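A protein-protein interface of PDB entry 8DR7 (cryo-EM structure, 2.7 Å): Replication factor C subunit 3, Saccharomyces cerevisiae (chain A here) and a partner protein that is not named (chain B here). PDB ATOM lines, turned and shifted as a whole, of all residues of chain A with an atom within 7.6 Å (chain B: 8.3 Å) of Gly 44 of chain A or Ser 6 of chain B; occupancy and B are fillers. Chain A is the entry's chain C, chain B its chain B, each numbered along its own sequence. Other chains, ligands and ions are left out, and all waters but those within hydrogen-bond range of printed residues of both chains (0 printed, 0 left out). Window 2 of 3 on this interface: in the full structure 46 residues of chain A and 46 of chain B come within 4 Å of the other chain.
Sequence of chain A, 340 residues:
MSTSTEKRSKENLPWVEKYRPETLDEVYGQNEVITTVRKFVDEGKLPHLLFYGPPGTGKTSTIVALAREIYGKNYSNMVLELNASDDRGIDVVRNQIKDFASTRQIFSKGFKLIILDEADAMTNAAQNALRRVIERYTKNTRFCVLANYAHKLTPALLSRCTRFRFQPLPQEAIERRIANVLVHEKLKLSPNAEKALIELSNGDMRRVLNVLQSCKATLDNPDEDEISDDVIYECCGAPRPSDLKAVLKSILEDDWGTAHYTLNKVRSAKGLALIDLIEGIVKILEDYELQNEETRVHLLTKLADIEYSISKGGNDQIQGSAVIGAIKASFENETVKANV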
ATOM      1  N   ARG A  38     -13.608  -0.673   0.796  1.00  0.00           N
ATOM      2  CA  ARG A  38     -14.661  -1.680   0.748  1.00  0.00           C
ATOM      3  C   ARG A  38     -14.705  -2.350  -0.617  1.00  0.00           C
ATOM      4  O   ARG A  38     -14.783  -3.581  -0.711  1.00  0.00           O
ATOM      5  CB  ARG A  38     -16.011  -1.044   1.075  1.00  0.00           C
ATOM      6  CG  ARG A  38     -17.180  -2.024   1.036  1.00  0.00           C
ATOM      7  CD  ARG A  38     -18.355  -1.588   1.910  1.00  0.00           C
ATOM      8  NE  ARG A  38     -17.947  -1.127   3.233  1.00  0.00           N
ATOM      9  CZ  ARG A  38     -18.697  -0.377   4.030  1.00  0.00           C
ATOM     10  NH1 ARG A  38     -19.911   0.014   3.674  1.00  0.00           N
ATOM     11  NH2 ARG A  38     -18.219  -0.011   5.215  1.00  0.00           N
ATOM     12  N   LYS A  39     -14.639  -1.559  -1.690  1.00  0.00           N
ATOM     13  CA  LYS A  39     -14.629  -2.137  -3.029  1.00  0.00           C
ATOM     14  C   LYS A  39     -13.394  -3.002  -3.242  1.00  0.00           C
ATOM     15  O   LYS A  39     -13.472  -4.066  -3.869  1.00  0.00           O
ATOM     16  CB  LYS A  39     -14.697  -1.028  -4.080  1.00  0.00           C
ATOM     17  CG  LYS A  39     -15.284  -1.473  -5.411  1.00  0.00           C
ATOM     18  CD  LYS A  39     -16.313  -0.479  -5.923  1.00  0.00           C
ATOM     19  CE  LYS A  39     -16.720  -0.778  -7.360  1.00  0.00           C
ATOM     20  NZ  LYS A  39     -16.685  -2.234  -7.675  1.00  0.00           N
ATOM     21  N   PHE A  40     -12.243  -2.561  -2.730  1.00  0.00           N
ATOM     22  CA  PHE A  40     -11.020  -3.342  -2.886  1.00  0.00           C
ATOM     23  C   PHE A  40     -11.144  -4.701  -2.210  1.00  0.00           C
ATOM     24  O   PHE A  40     -10.730  -5.722  -2.771  1.00  0.00           O
ATOM     25  CB  PHE A  40      -9.829  -2.573  -2.307  1.00  0.00           C
ATOM     26  CG  PHE A  40      -9.319  -1.459  -3.188  1.00  0.00           C
ATOM     27  CD1 PHE A  40      -9.870  -1.211  -4.438  1.00  0.00           C
ATOM     28  CD2 PHE A  40      -8.274  -0.659  -2.757  1.00  0.00           C
ATOM     29  CE1 PHE A  40      -9.390  -0.189  -5.232  1.00  0.00           C
ATOM     30  CE2 PHE A  40      -7.791   0.365  -3.549  1.00  0.00           C
ATOM     31  CZ  PHE A  40      -8.350   0.600  -4.787  1.00  0.00           C
ATOM     32  N   VAL A  41     -11.710  -4.736  -1.004  1.00  0.00           N
ATOM     33  CA  VAL A  41     -11.761  -5.971  -0.228  1.00  0.00           C
ATOM     34  C   VAL A  41     -12.956  -6.822  -0.644  1.00  0.00           C
ATOM     35  O   VAL A  41     -13.048  -7.996  -0.270  1.00  0.00           O
ATOM     36  CB  VAL A  41     -11.801  -5.678   1.285  1.00  0.00           C
ATOM     37  CG1 VAL A  41     -10.600  -4.840   1.697  1.00  0.00           C
ATOM     38  CG2 VAL A  41     -13.102  -4.985   1.668  1.00  0.00           C
ATOM     39  N   ASP A  42     -13.879  -6.247  -1.418  1.00  0.00           N
ATOM     40  CA  ASP A  42     -15.031  -7.001  -1.893  1.00  0.00           C
ATOM     41  C   ASP A  42     -14.763  -7.794  -3.165  1.00  0.00           C
ATOM     42  O   ASP A  42     -15.555  -8.684  -3.493  1.00  0.00           O
ATOM     43  CB  ASP A  42     -16.217  -6.061  -2.147  1.00  0.00           C
ATOM     44  CG  ASP A  42     -17.500  -6.558  -1.512  1.00  0.00           C
ATOM     45  OD1 ASP A  42     -18.171  -5.763  -0.822  1.00  0.00           O
ATOM     46  OD2 ASP A  42     -17.839  -7.745  -1.705  1.00  0.00           O
ATOM     47  N   GLU A  43     -13.678  -7.501  -3.888  1.00  0.00           N
ATOM     48  CA  GLU A  43     -13.396  -8.176  -5.149  1.00  0.00           C
ATOM     49  C   GLU A  43     -11.947  -8.636  -5.273  1.00  0.00           C
ATOM     50  O   GLU A  43     -11.519  -8.993  -6.377  1.00  0.00           O
ATOM     51  CB  GLU A  43     -13.771  -7.270  -6.330  1.00  0.00           C
ATOM     52  CG  GLU A  43     -13.061  -5.924  -6.359  1.00  0.00           C
ATOM     53  CD  GLU A  43     -12.044  -5.811  -7.478  1.00  0.00           C
ATOM     54  OE1 GLU A  43     -12.249  -6.426  -8.546  1.00  0.00           O
ATOM     55  OE2 GLU A  43     -11.042  -5.091  -7.294  1.00  0.00           O
ATOM     56  N   GLY A  44     -11.184  -8.640  -4.180  1.00  0.00           N
ATOM     57  CA  GLY A  44      -9.906  -9.317  -4.134  1.00  0.00           C
ATOM     58  C   GLY A  44      -8.704  -8.502  -4.563  1.00  0.00           C
ATOM     59  O   GLY A  44      -7.572  -8.970  -4.392  1.00  0.00           O
ATOM     60  N   LYS A  45      -8.901  -7.303  -5.110  1.00  0.00           N
ATOM     61  CA  LYS A  45      -7.789  -6.458  -5.547  1.00  0.00           C
ATOM     62  C   LYS A  45      -7.476  -5.460  -4.436  1.00  0.00           C
ATOM     63  O   LYS A  45      -7.927  -4.316  -4.436  1.00  0.00           O
ATOM     64  CB  LYS A  45      -8.121  -5.761  -6.862  1.00  0.00           C
ATOM     65  CG  LYS A  45      -8.667  -6.688  -7.939  1.00  0.00           C
ATOM     66  CD  LYS A  45      -8.748  -5.986  -9.290  1.00  0.00           C
ATOM     67  CE  LYS A  45      -8.504  -6.942 -10.450  1.00  0.00           C
ATOM     68  NZ  LYS A  45      -7.147  -7.556 -10.413  1.00  0.00           N
ATOM     69  N   LEU A  46      -6.681  -5.918  -3.471  1.00  0.00           N
ATOM     70  CA  LEU A  46      -6.257  -5.085  -2.352  1.00  0.00           C
ATOM     71  C   LEU A  46      -4.775  -4.769  -2.498  1.00  0.00           C
ATOM     72  O   LEU A  46      -3.935  -5.651  -2.256  1.00  0.00           O
ATOM     73  CB  LEU A  46      -6.528  -5.796  -1.023  1.00  0.00           C
ATOM     74  CG  LEU A  46      -5.746  -5.340   0.214  1.00  0.00           C
ATOM     75  CD1 LEU A  46      -6.200  -3.959   0.654  1.00  0.00           C
ATOM     76  CD2 LEU A  46      -5.917  -6.343   1.341  1.00  0.00           C
ATOM     77  N   PRO A  47      -4.396  -3.547  -2.890  1.00  0.00           N
ATOM     78  CA  PRO A  47      -2.969  -3.230  -3.020  1.00  0.00           C
ATOM     79  C   PRO A  47      -2.346  -2.797  -1.705  1.00  0.00           C
ATOM     80  O   PRO A  47      -3.029  -2.727  -0.678  1.00  0.00           O
ATOM     81  CB  PRO A  47      -2.968  -2.091  -4.044  1.00  0.00           C
ATOM     82  CG  PRO A  47      -4.248  -1.372  -3.772  1.00  0.00           C
ATOM     83  CD  PRO A  47      -5.245  -2.421  -3.318  1.00  0.00           C
ATOM     84  N   GLY A 110      -5.636 -18.100   4.093  1.00  0.00           N
ATOM     85  CA  GLY A 110      -5.762 -16.690   3.792  1.00  0.00           C
ATOM     86  C   GLY A 110      -4.406 -16.091   3.487  1.00  0.00           C
ATOM     87  O   GLY A 110      -3.370 -16.758   3.569  1.00  0.00           O
ATOM     88  N   PHE A 111      -4.434 -14.811   3.134  1.00  0.00           N
ATOM     89  CA  PHE A 111      -3.217 -14.078   2.828  1.00  0.00           C
ATOM     90  C   PHE A 111      -2.689 -13.380   4.078  1.00  0.00           C
ATOM     91  O   PHE A 111      -3.417 -13.137   5.042  1.00  0.00           O
ATOM     92  CB  PHE A 111      -3.462 -13.057   1.715  1.00  0.00           C
ATOM     93  CG  PHE A 111      -4.333 -11.903   2.124  1.00  0.00           C
ATOM     94  CD1 PHE A 111      -5.711 -11.993   2.039  1.00  0.00           C
ATOM     95  CD2 PHE A 111      -3.771 -10.726   2.590  1.00  0.00           C
ATOM     96  CE1 PHE A 111      -6.513 -10.933   2.412  1.00  0.00           C
ATOM     97  CE2 PHE A 111      -4.568  -9.662   2.965  1.00  0.00           C
ATOM     98  CZ  PHE A 111      -5.939  -9.765   2.874  1.00  0.00           C
ATOM     99  N   LYS A 139       2.543 -11.578  -3.890  1.00  0.00           N
ATOM    100  CA  LYS A 139       1.496 -12.511  -4.293  1.00  0.00           C
ATOM    101  C   LYS A 139       0.637 -12.929  -3.106  1.00  0.00           C
ATOM    102  O   LYS A 139      -0.591 -13.022  -3.222  1.00  0.00           O
ATOM    103  CB  LYS A 139       2.118 -13.738  -4.961  1.00  0.00           C
ATOM    104  CG  LYS A 139       1.105 -14.698  -5.574  1.00  0.00           C
ATOM    105  CD  LYS A 139       1.607 -16.132  -5.547  1.00  0.00           C
ATOM    106  CE  LYS A 139       0.521 -17.111  -5.966  1.00  0.00           C
ATOM    107  NZ  LYS A 139       0.423 -17.240  -7.447  1.00  0.00           N
ATOM    108  N   ARG A 142       0.440  -8.476   1.811  1.00  0.00           N
ATOM    109  CA  ARG A 142       0.144  -7.078   1.543  1.00  0.00           C
ATOM    110  C   ARG A 142       0.600  -6.236   2.726  1.00  0.00           C
ATOM    111  O   ARG A 142       0.591  -6.693   3.872  1.00  0.00           O
ATOM    112  CB  ARG A 142      -1.353  -6.858   1.282  1.00  0.00           C
ATOM    113  CG  ARG A 142      -1.831  -7.373  -0.068  1.00  0.00           C
ATOM    114  CD  ARG A 142      -1.136  -6.663  -1.220  1.00  0.00           C
ATOM    115  NE  ARG A 142      -1.846  -6.839  -2.482  1.00  0.00           N
ATOM    116  CZ  ARG A 142      -1.734  -7.903  -3.266  1.00  0.00           C
ATOM    117  NH1 ARG A 142      -0.936  -8.913  -2.954  1.00  0.00           N
ATOM    118  NH2 ARG A 142      -2.438  -7.956  -4.392  1.00  0.00           N
ATOM    119  N   THR B   4     -13.135 -14.514  -0.453  1.00  0.00           N
ATOM    120  CA  THR B   4     -12.787 -13.122  -0.197  1.00  0.00           C
ATOM    121  C   THR B   4     -11.340 -12.988   0.270  1.00  0.00           C
ATOM    122  O   THR B   4     -10.909 -11.905   0.669  1.00  0.00           O
ATOM    123  CB  THR B   4     -13.713 -12.498   0.865  1.00  0.00           C
ATOM    124  OG1 THR B   4     -13.683 -13.293   2.058  1.00  0.00           O
ATOM    125  CG2 THR B   4     -15.141 -12.415   0.348  1.00  0.00           C
ATOM    126  N   LEU B   5     -10.592 -14.092   0.218  1.00  0.00           N
ATOM    127  CA  LEU B   5      -9.195 -14.110   0.633  1.00  0.00           C
ATOM    128  C   LEU B   5      -8.253 -14.480  -0.506  1.00  0.00           C
ATOM    129  O   LEU B   5      -7.078 -14.774  -0.252  1.00  0.00           O
ATOM    130  CB  LEU B   5      -9.004 -15.082   1.802  1.00  0.00           C
ATOM    131  CG  LEU B   5      -9.816 -14.772   3.062  1.00  0.00           C
ATOM    132  CD1 LEU B   5      -9.746 -15.931   4.043  1.00  0.00           C
ATOM    133  CD2 LEU B   5      -9.330 -13.486   3.714  1.00  0.00           C
ATOM    134  N   SER B   6      -8.730 -14.474  -1.748  1.00  0.00           N
ATOM    135  CA  SER B   6      -7.910 -14.792  -2.915  1.00  0.00           C
ATOM    136  C   SER B   6      -7.457 -13.475  -3.538  1.00  0.00           C
ATOM    137  O   SER B   6      -8.201 -12.841  -4.290  1.00  0.00           O
ATOM    138  CB  SER B   6      -8.688 -15.646  -3.910  1.00  0.00           C
ATOM    139  OG  SER B   6      -9.918 -15.032  -4.255  1.00  0.00           O
ATOM    140  N   LEU B   7      -6.232 -13.066  -3.221  1.00  0.00           N
ATOM    141  CA  LEU B   7      -5.706 -11.809  -3.729  1.00  0.00           C
ATOM    142  C   LEU B   7      -5.381 -11.918  -5.214  1.00  0.00           C
ATOM    143  O   LEU B   7      -4.954 -12.966  -5.709  1.00  0.00           O
ATOM    144  CB  LEU B   7      -4.451 -11.403  -2.955  1.00  0.00           C
ATOM    145  CG  LEU B   7      -4.652 -10.791  -1.568  1.00  0.00           C
ATOM    146  CD1 LEU B   7      -3.304 -10.542  -0.914  1.00  0.00           C
ATOM    147  CD2 LEU B   7      -5.455  -9.500  -1.638  1.00  0.00           C
ATOM    148  N   GLN B   8      -5.589 -10.815  -5.927  1.00  0.00           N
ATOM    149  CA  GLN B   8      -5.250 -10.712  -7.338  1.00  0.00           C
ATOM    150  C   GLN B   8      -3.894 -10.035  -7.485  1.00  0.00           C
ATOM    151  O   GLN B   8      -3.606  -9.045  -6.807  1.00  0.00           O
ATOM    152  CB  GLN B   8      -6.316  -9.923  -8.100  1.00  0.00           C
ATOM    153  CG  GLN B   8      -7.714 -10.513  -8.004  1.00  0.00           C
ATOM    154  CD  GLN B   8      -7.804 -11.905  -8.599  1.00  0.00           C
ATOM    155  OE1 GLN B   8      -8.228 -12.851  -7.935  1.00  0.00           O
ATOM    156  NE2 GLN B   8      -7.408 -12.035  -9.860  1.00  0.00           N
ATOM    157  N   LEU B   9      -3.066 -10.576  -8.368  1.00  0.00           N
ATOM    158  CA  LEU B   9      -1.715 -10.057  -8.531  1.00  0.00           C
ATOM    159  C   LEU B   9      -1.768  -8.614  -9.025  1.00  0.00           C
ATOM    160  O   LEU B   9      -2.448  -8.331 -10.019  1.00  0.00           O
ATOM    161  CB  LEU B   9      -0.929 -10.924  -9.514  1.00  0.00           C
ATOM    162  CG  LEU B   9       0.588 -10.732  -9.514  1.00  0.00           C
ATOM    163  CD1 LEU B   9       1.198 -11.189  -8.198  1.00  0.00           C
ATOM    164  CD2 LEU B   9       1.216 -11.476 -10.682  1.00  0.00           C
ATOM    165  N   PRO B  10      -1.078  -7.678  -8.371  1.00  0.00           N
ATOM    166  CA  PRO B  10      -1.081  -6.296  -8.861  1.00  0.00           C
ATOM    167  C   PRO B  10      -0.458  -6.188 -10.244  1.00  0.00           C
ATOM    168  O   PRO B  10       0.421  -6.966 -10.620  1.00  0.00           O
ATOM    169  CB  PRO B  10      -0.250  -5.541  -7.816  1.00  0.00           C
ATOM    170  CG  PRO B  10      -0.277  -6.401  -6.605  1.00  0.00           C
ATOM    171  CD  PRO B  10      -0.327  -7.805  -7.110  1.00  0.00           C
ATOM    172  N   GLN B 210      -4.592   1.294 -11.586  1.00  0.00           N
ATOM    173  CA  GLN B 210      -5.338   0.175 -11.020  1.00  0.00           C
ATOM    174  C   GLN B 210      -6.366   0.650 -10.001  1.00  0.00           C
ATOM    175  O   GLN B 210      -7.534   0.239 -10.055  1.00  0.00           O
ATOM    176  CB  GLN B 210      -4.373  -0.824 -10.380  1.00  0.00           C
ATOM    177  CG  GLN B 210      -4.950  -2.221 -10.211  1.00  0.00           C
ATOM    178  CD  GLN B 210      -3.882  -3.265  -9.954  1.00  0.00           C
ATOM    179  OE1 GLN B 210      -2.728  -2.936  -9.681  1.00  0.00           O
ATOM    180  NE2 GLN B 210      -4.262  -4.534 -10.043  1.00  0.00           N
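The backbone NH (N) of Gln 8 of chain B lies within hydrogen-bond range of the backbone carbonyl oxygen (O) of Gly 44 of chain A (3.1 Å).
The backbone carbonyl oxygen (O) of Gln 8 of chain B sits at hydrogen-bond distance from the guanidinium group (NH2) of Arg 142 of chain A.
O of Phe 40 of chain A lies within hydrogen-bond range of N of Lys 45 of chain A, at 3.4 Å.
The backbone carbonyl oxygen (O) of Leu 46 of chain A lies within hydrogen-bond range of the guanidinium group (NE) of Arg 142 of chain A (2.4 Å).
Among the printed residues, pairs that only touch across the chains: Gly 44 of chain A with Ser 6 of chain B (3.9 Å), Gly 44 of chain A with Leu 7 of chain B (3.5 Å), Lys 45 of chain A with Gln 8 of chain B (3.4 Å), Leu 46 of chain A with Leu 7 of chain B (3.9 Å), Phe 111 of chain A with Leu 5 of chain B (3.9 Å), Phe 111 of chain A with Leu 7 of chain B (3.5 Å), Arg 142 of chain A with Leu 7 of chain B (3.5 Å) and Arg 142 of chain A with Pro 10 of chain B (3.4 Å).
Of chain B, only Ser 6 (3.9 Å), Leu 7 (3.5 Å) and Gln 8 (3.1 Å) come within 4 Å of Gly 44 of chain A.
Of the printed residues of chain B, Lys 45 of chain A touches Gln 8.
Printed residues of chain B within 4 Å of Phe 111 of chain A: Leu 5 and Leu 7.
Of the printed residues of chain A, Leu 5 of chain B touches Phe 111.
Of chain A, only Gly 44 (3.9 Å) comes within 4 Å of Ser 6 of chain B.
Of the printed residues of chain A, Gln 8 of chain B touches Gly 44, Lys 45 and Arg 142.
The nearest residue of chain B that does not touch Gly 44 of chain A is Thr 4 of chain B (5.5 Å).
Printed residues of chain A that touch a printed residue of chain B: Gly 44, Lys 45, Leu 46, Phe 111 and Arg 142.
Hydrophobic or aromatic side chains of chain A within 4 Å of the printed part of chain B: Leu 46 and Phe 111.
Printed residues of chain B that touch a printed residue of chain A: Leu 5, Ser 6, Leu 7, Gln 8 and Pro 10.
Hydrophobic or aromatic side chains of chain B that line the printed part of chain A: Leu 7 and Pro 10.
Among the printed residues, no Asp or Glu carboxylate lies within 4 Å of a Lys or Arg side-chain nitrogen of the other chain.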
